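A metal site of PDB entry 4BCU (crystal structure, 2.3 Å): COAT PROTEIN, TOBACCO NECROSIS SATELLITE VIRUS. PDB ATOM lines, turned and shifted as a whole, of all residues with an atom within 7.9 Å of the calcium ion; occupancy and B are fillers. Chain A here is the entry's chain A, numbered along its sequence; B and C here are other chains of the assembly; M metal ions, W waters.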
ATOM      1  N   LYS A  28     -16.671   2.756   7.916  1.00  0.00           N
ATOM      2  CA  LYS A  28     -16.201   1.391   8.125  1.00  0.00           C
ATOM      3  C   LYS A  28     -17.360   0.410   8.042  1.00  0.00           C
ATOM      4  O   LYS A  28     -18.526   0.842   8.121  1.00  0.00           O
ATOM      5  CB  LYS A  28     -15.409   1.298   9.426  1.00  0.00           C
ATOM      6  CG  LYS A  28     -14.063   2.002   9.262  1.00  0.00           C
ATOM      7  CD  LYS A  28     -13.289   1.949  10.610  1.00  0.00           C
ATOM      8  CE  LYS A  28     -11.932   2.672  10.530  1.00  0.00           C
ATOM      9  NZ  LYS A  28     -11.150   2.664  11.872  1.00  0.00           N
ATOM     10  N   GLN A  60     -12.517  -3.025  11.642  1.00  0.00           N
ATOM     11  CA  GLN A  60     -12.027  -2.929  13.026  1.00  0.00           C
ATOM     12  C   GLN A  60     -12.348  -1.534  13.589  1.00  0.00           C
ATOM     13  O   GLN A  60     -13.182  -0.789  12.972  1.00  0.00           O
ATOM     14  CB  GLN A  60     -10.513  -3.238  13.053  1.00  0.00           C
ATOM     15  CG  GLN A  60     -10.267  -4.685  12.568  1.00  0.00           C
ATOM     16  CD  GLN A  60      -8.829  -5.155  12.583  1.00  0.00           C
ATOM     17  OE1 GLN A  60      -7.918  -4.385  12.323  1.00  0.00           O
ATOM     18  NE2 GLN A  60      -8.638  -6.448  12.825  1.00  0.00           N
ATOM     19  N   ARG A  61     -11.727  -1.159  14.718  1.00  0.00           N
ATOM     20  CA  ARG A  61     -11.963   0.149  15.354  1.00  0.00           C
ATOM     21  C   ARG A  61     -10.751   0.658  16.126  1.00  0.00           C
ATOM     22  O   ARG A  61      -9.910  -0.123  16.633  1.00  0.00           O
ATOM     23  CB  ARG A  61     -13.131   0.078  16.354  1.00  0.00           C
ATOM     24  CG  ARG A  61     -12.911  -0.925  17.522  1.00  0.00           C
ATOM     25  CD  ARG A  61     -14.149  -1.106  18.470  1.00  0.00           C
ATOM     26  NE  ARG A  61     -14.046  -2.402  19.123  1.00  0.00           N
ATOM     27  CZ  ARG A  61     -13.467  -2.602  20.320  1.00  0.00           C
ATOM     28  NH1 ARG A  61     -12.938  -1.588  21.010  1.00  0.00           N
ATOM     29  NH2 ARG A  61     -13.411  -3.819  20.815  1.00  0.00           N
ATOM     30  N   SER A  62     -10.698   1.988  16.241  1.00  0.00           N
ATOM     31  CA  SER A  62      -9.767   2.690  17.107  1.00  0.00           C
ATOM     32  C   SER A  62     -10.506   2.980  18.421  1.00  0.00           C
ATOM     33  O   SER A  62     -11.656   3.422  18.384  1.00  0.00           O
ATOM     34  CB  SER A  62      -9.481   4.030  16.421  1.00  0.00           C
ATOM     35  OG  SER A  62      -8.413   4.677  17.053  1.00  0.00           O
ATOM     36  N   GLY A  63      -9.881   2.763  19.573  1.00  0.00           N
ATOM     37  CA  GLY A  63     -10.557   3.092  20.854  1.00  0.00           C
ATOM     38  C   GLY A  63     -11.752   2.192  21.191  1.00  0.00           C
ATOM     39  O   GLY A  63     -11.886   1.043  20.707  1.00  0.00           O
ATOM     40  N   ASP A  64     -12.648   2.707  22.003  1.00  0.00           N
ATOM     41  CA  ASP A  64     -13.710   1.900  22.568  1.00  0.00           C
ATOM     42  C   ASP A  64     -15.071   2.444  22.168  1.00  0.00           C
ATOM     43  O   ASP A  64     -16.098   2.033  22.758  1.00  0.00           O
ATOM     44  CB  ASP A  64     -13.560   1.757  24.122  1.00  0.00           C
ATOM     45  CG  ASP A  64     -12.461   0.750  24.514  1.00  0.00           C
ATOM     46  OD1 ASP A  64     -12.108  -0.178  23.706  1.00  0.00           O
ATOM     47  OD2 ASP A  64     -11.918   0.856  25.647  1.00  0.00           O
ATOM     48  N   GLN A  65     -15.112   3.296  21.137  1.00  0.00           N
ATOM     49  CA  GLN A  65     -16.406   3.676  20.615  1.00  0.00           C
ATOM     50  C   GLN A  65     -16.419   3.609  19.116  1.00  0.00           C
ATOM     51  O   GLN A  65     -15.406   3.851  18.476  1.00  0.00           O
ATOM     52  CB  GLN A  65     -16.923   5.070  21.075  1.00  0.00           C
ATOM     53  CG  GLN A  65     -16.825   5.410  22.565  1.00  0.00           C
ATOM     54  CD  GLN A  65     -17.464   6.781  22.852  1.00  0.00           C
ATOM     55  OE1 GLN A  65     -17.263   7.719  22.107  1.00  0.00           O
ATOM     56  NE2 GLN A  65     -18.256   6.877  23.922  1.00  0.00           N
ATOM     57  N   VAL A  66     -17.586   3.267  18.572  1.00  0.00           N
ATOM     58  CA  VAL A  66     -17.892   3.460  17.153  1.00  0.00           C
ATOM     59  C   VAL A  66     -19.323   3.980  17.097  1.00  0.00           C
ATOM     60  O   VAL A  66     -20.053   3.937  18.077  1.00  0.00           O
ATOM     61  CB  VAL A  66     -17.759   2.130  16.297  1.00  0.00           C
ATOM     62  CG1 VAL A  66     -16.430   1.509  16.502  1.00  0.00           C
ATOM     63  CG2 VAL A  66     -18.829   1.088  16.675  1.00  0.00           C
ATOM     64  N   ARG A  67     -19.741   4.492  15.962  1.00  0.00           N
ATOM     65  CA  ARG A  67     -21.120   4.906  15.885  1.00  0.00           C
ATOM     66  C   ARG A  67     -21.770   4.188  14.673  1.00  0.00           C
ATOM     67  O   ARG A  67     -21.381   4.399  13.565  1.00  0.00           O
ATOM     68  CB  ARG A  67     -21.174   6.445  15.838  1.00  0.00           C
ATOM     69  CG  ARG A  67     -22.479   7.016  15.405  1.00  0.00           C
ATOM     70  CD  ARG A  67     -22.463   8.592  15.476  1.00  0.00           C
ATOM     71  NE  ARG A  67     -22.098   9.039  16.829  1.00  0.00           N
ATOM     72  CZ  ARG A  67     -23.006   9.219  17.786  1.00  0.00           C
ATOM     73  NH1 ARG A  67     -24.286   9.015  17.486  1.00  0.00           N
ATOM     74  NH2 ARG A  67     -22.641   9.594  19.024  1.00  0.00           N
ATOM     75  N   VAL A 155     -21.969   2.746  20.049  1.00  0.00           N
ATOM     76  CA  VAL A 155     -21.640   1.460  20.687  1.00  0.00           C
ATOM     77  C   VAL A 155     -20.344   1.689  21.479  1.00  0.00           C
ATOM     78  O   VAL A 155     -19.341   2.059  20.862  1.00  0.00           O
ATOM     79  CB  VAL A 155     -21.340   0.340  19.618  1.00  0.00           C
ATOM     80  CG1 VAL A 155     -20.808  -0.939  20.337  1.00  0.00           C
ATOM     81  CG2 VAL A 155     -22.582   0.018  18.836  1.00  0.00           C
ATOM     82  N   TYR A 157     -17.322  -0.046  23.896  1.00  0.00           N
ATOM     83  CA  TYR A 157     -16.658  -1.303  24.239  1.00  0.00           C
ATOM     84  C   TYR A 157     -15.949  -1.235  25.622  1.00  0.00           C
ATOM     85  O   TYR A 157     -15.591  -0.139  26.073  1.00  0.00           O
ATOM     86  CB  TYR A 157     -15.645  -1.744  23.128  1.00  0.00           C
ATOM     87  CG  TYR A 157     -16.372  -2.113  21.852  1.00  0.00           C
ATOM     88  CD1 TYR A 157     -16.888  -1.144  21.041  1.00  0.00           C
ATOM     89  CD2 TYR A 157     -16.633  -3.457  21.518  1.00  0.00           C
ATOM     90  CE1 TYR A 157     -17.560  -1.458  19.864  1.00  0.00           C
ATOM     91  CE2 TYR A 157     -17.348  -3.794  20.339  1.00  0.00           C
ATOM     92  CZ  TYR A 157     -17.786  -2.772  19.508  1.00  0.00           C
ATOM     93  OH  TYR A 157     -18.519  -3.023  18.342  1.00  0.00           O
ATOM     94  N   TYR A 193     -20.428   1.853  10.028  1.00  0.00           N
ATOM     95  CA  TYR A 193     -20.172   2.677  11.229  1.00  0.00           C
ATOM     96  C   TYR A 193     -19.057   3.694  11.068  1.00  0.00           C
ATOM     97  O   TYR A 193     -18.114   3.443  10.334  1.00  0.00           O
ATOM     98  CB  TYR A 193     -19.863   1.776  12.413  1.00  0.00           C
ATOM     99  CG  TYR A 193     -18.637   0.897  12.239  1.00  0.00           C
ATOM    100  CD1 TYR A 193     -18.718  -0.336  11.591  1.00  0.00           C
ATOM    101  CD2 TYR A 193     -17.418   1.282  12.791  1.00  0.00           C
ATOM    102  CE1 TYR A 193     -17.624  -1.170  11.452  1.00  0.00           C
ATOM    103  CE2 TYR A 193     -16.299   0.487  12.697  1.00  0.00           C
ATOM    104  CZ  TYR A 193     -16.383  -0.756  12.001  1.00  0.00           C
ATOM    105  OH  TYR A 193     -15.244  -1.562  11.887  1.00  0.00           O
ATOM    106  N   THR A 194     -19.133   4.847  11.742  1.00  0.00           N
ATOM    107  CA  THR A 194     -18.009   5.772  11.697  1.00  0.00           C
ATOM    108  C   THR A 194     -17.195   5.534  12.961  1.00  0.00           C
ATOM    109  O   THR A 194     -17.682   4.889  13.913  1.00  0.00           O
ATOM    110  CB  THR A 194     -18.442   7.251  11.611  1.00  0.00           C
ATOM    111  OG1 THR A 194     -19.332   7.574  12.708  1.00  0.00           O
ATOM    112  CG2 THR A 194     -19.139   7.516  10.264  1.00  0.00           C
ATOM    113  N   ASP A 195     -15.987   6.078  12.999  1.00  0.00           N
ATOM    114  CA  ASP A 195     -15.060   5.691  14.047  1.00  0.00           C
ATOM    115  C   ASP A 195     -14.094   6.830  14.269  1.00  0.00           C
ATOM    116  O   ASP A 195     -12.915   6.590  14.365  1.00  0.00           O
ATOM    117  CB  ASP A 195     -14.311   4.390  13.630  1.00  0.00           C
ATOM    118  CG  ASP A 195     -13.287   3.934  14.672  1.00  0.00           C
ATOM    119  OD1 ASP A 195     -13.450   4.242  15.876  1.00  0.00           O
ATOM    120  OD2 ASP A 195     -12.303   3.295  14.300  1.00  0.00           O
ATOM    121  N   ALA A 196     -14.575   8.058  14.404  1.00  0.00           N
ATOM    122  CA  ALA A 196     -13.682   9.242  14.389  1.00  0.00           C
ATOM    123  C   ALA A 196     -13.180   9.750  15.767  1.00  0.00           C
ATOM    124  O   ALA A 196     -13.666   9.257  16.790  1.00  0.00           O
ATOM    125  CB  ALA A 196     -14.367  10.348  13.678  1.00  0.00           C
ATOM    126  N   HIS B  24     -19.677  13.367  17.337  1.00  0.00           N
ATOM    127  CA  HIS B  24     -19.162  12.450  16.326  1.00  0.00           C
ATOM    128  C   HIS B  24     -17.745  11.913  16.549  1.00  0.00           C
ATOM    129  O   HIS B  24     -17.296  11.000  15.821  1.00  0.00           O
ATOM    130  CB  HIS B  24     -19.259  13.143  14.968  1.00  0.00           C
ATOM    131  CG  HIS B  24     -20.639  13.078  14.404  1.00  0.00           C
ATOM    132  ND1 HIS B  24     -21.562  14.084  14.593  1.00  0.00           N
ATOM    133  CD2 HIS B  24     -21.279  12.089  13.740  1.00  0.00           C
ATOM    134  CE1 HIS B  24     -22.710  13.729  14.048  1.00  0.00           C
ATOM    135  NE2 HIS B  24     -22.565  12.518  13.521  1.00  0.00           N
ATOM    136  N   LEU B  25     -17.047  12.464  17.540  1.00  0.00           N
ATOM    137  CA  LEU B  25     -15.638  12.100  17.768  1.00  0.00           C
ATOM    138  C   LEU B  25     -15.528  11.296  19.054  1.00  0.00           C
ATOM    139  O   LEU B  25     -16.138  11.665  20.034  1.00  0.00           O
ATOM    140  CB  LEU B  25     -14.719  13.343  17.836  1.00  0.00           C
ATOM    141  CG  LEU B  25     -14.886  14.381  16.728  1.00  0.00           C
ATOM    142  CD1 LEU B  25     -14.055  15.712  16.974  1.00  0.00           C
ATOM    143  CD2 LEU B  25     -14.692  13.740  15.322  1.00  0.00           C
ATOM    144  N   GLU B  26     -14.730  10.239  19.079  1.00  0.00           N
ATOM    145  CA  GLU B  26     -14.512   9.541  20.315  1.00  0.00           C
ATOM    146  C   GLU B  26     -13.741  10.416  21.286  1.00  0.00           C
ATOM    147  O   GLU B  26     -12.678  10.959  20.921  1.00  0.00           O
ATOM    148  CB  GLU B  26     -13.762   8.209  20.109  1.00  0.00           C
ATOM    149  CG  GLU B  26     -13.569   7.448  21.461  1.00  0.00           C
ATOM    150  CD  GLU B  26     -13.047   6.015  21.281  1.00  0.00           C
ATOM    151  OE1 GLU B  26     -13.290   5.404  20.217  1.00  0.00           O
ATOM    152  OE2 GLU B  26     -12.433   5.465  22.234  1.00  0.00           O
ATOM    153  N   HIS B  27     -14.248  10.562  22.502  1.00  0.00           N
ATOM    154  CA  HIS B  27     -13.446  11.185  23.538  1.00  0.00           C
ATOM    155  C   HIS B  27     -12.652  10.132  24.286  1.00  0.00           C
ATOM    156  O   HIS B  27     -13.158   9.523  25.243  1.00  0.00           O
ATOM    157  CB  HIS B  27     -14.313  11.976  24.507  1.00  0.00           C
ATOM    158  CG  HIS B  27     -14.928  13.164  23.879  1.00  0.00           C
ATOM    159  ND1 HIS B  27     -15.454  13.130  22.592  1.00  0.00           N
ATOM    160  CD2 HIS B  27     -15.089  14.428  24.320  1.00  0.00           C
ATOM    161  CE1 HIS B  27     -15.906  14.326  22.285  1.00  0.00           C
ATOM    162  NE2 HIS B  27     -15.679  15.136  23.310  1.00  0.00           N
ATOM    163  N   LYS B  28     -11.434   9.910  23.795  1.00  0.00           N
ATOM    164  CA  LYS B  28     -10.405   9.076  24.404  1.00  0.00           C
ATOM    165  C   LYS B  28      -9.995   9.638  25.746  1.00  0.00           C
ATOM    166  O   LYS B  28     -10.279  10.818  26.035  1.00  0.00           O
ATOM    167  CB  LYS B  28      -9.252   8.859  23.438  1.00  0.00           C
ATOM    168  CG  LYS B  28      -9.685   7.940  22.296  1.00  0.00           C
ATOM    169  CD  LYS B  28      -8.510   7.789  21.285  1.00  0.00           C
ATOM    170  CE  LYS B  28      -8.896   6.887  20.091  1.00  0.00           C
ATOM    171  NZ  LYS B  28      -7.758   6.730  19.046  1.00  0.00           N
ATOM    172  N   ASP B  56      -4.102   1.464  19.206  1.00  0.00           N
ATOM    173  CA  ASP B  56      -5.540   1.489  19.024  1.00  0.00           C
ATOM    174  C   ASP B  56      -6.397   1.474  20.280  1.00  0.00           C
ATOM    175  O   ASP B  56      -7.624   1.368  20.165  1.00  0.00           O
ATOM    176  CB  ASP B  56      -5.948   0.299  18.161  1.00  0.00           C
ATOM    177  CG  ASP B  56      -5.199   0.278  16.864  1.00  0.00           C
ATOM    178  OD1 ASP B  56      -5.281   1.290  16.075  1.00  0.00           O
ATOM    179  OD2 ASP B  56      -4.533  -0.764  16.646  1.00  0.00           O
ATOM    180  N   GLN C 122     -15.844   6.981  30.104  1.00  0.00           N
ATOM    181  CA  GLN C 122     -16.132   7.271  28.696  1.00  0.00           C
ATOM    182  C   GLN C 122     -17.576   6.891  28.334  1.00  0.00           C
ATOM    183  O   GLN C 122     -18.260   7.688  27.695  1.00  0.00           O
ATOM    184  CB  GLN C 122     -15.177   6.524  27.747  1.00  0.00           C
ATOM    185  CG  GLN C 122     -15.483   6.806  26.275  1.00  0.00           C
ATOM    186  CD  GLN C 122     -14.651   5.976  25.337  1.00  0.00           C
ATOM    187  OE1 GLN C 122     -14.820   4.725  25.249  1.00  0.00           O
ATOM    188  NE2 GLN C 122     -13.713   6.638  24.643  1.00  0.00           N
HETATM  189 CA    CA M   1     -13.409   4.879  17.936  1.00  0.00          CA
HETATM  190  O   HOH W   1     -14.910   6.636  17.365  1.00  0.00           O
HETATM  191  O   HOH W   2     -11.985   6.377  17.078  1.00  0.00           O
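The side-chain carboxylate of Asp 195 lies within salt-bridge range of the side-chain amino group of Lys 28 of chain A (2.8 Å). OG of Ser 62 sits at hydrogen-bond distance from NZ of Lys 28 of chain B, 2.9 Å away. N of Glu 26 of chain B sits at hydrogen-bond distance from O of Ala 196 (2.7 Å). The side-chain carboxylate (OE2) of Glu 26 of chain B lies within hydrogen-bond range of the backbone NH (N) of Asp 64 (2.8 Å). OE2 of Glu 26 of chain B is in hydrogen-bond range of NE2 of Gln 122 of chain C.
The calcium ion is bound by OD1 of Asp 195, at 2.2 Å. The calcium ion is bound by water W2 (2.2 Å). O of Gln 65 binds the calcium ion. The backbone carbonyl oxygen (O) of Ser 62 binds the calcium ion. The calcium ion is bound by the side-chain carboxylate (OE1) of Glu 26 of chain B (2.3 Å). The calcium ion is bound by water W1 (2.4 Å).
Of the 22 residues printed, 4 come within 4 Å of the calcium ion. The nearest printed residue that does not touch the calcium ion is Gly 63 (4.4 Å).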
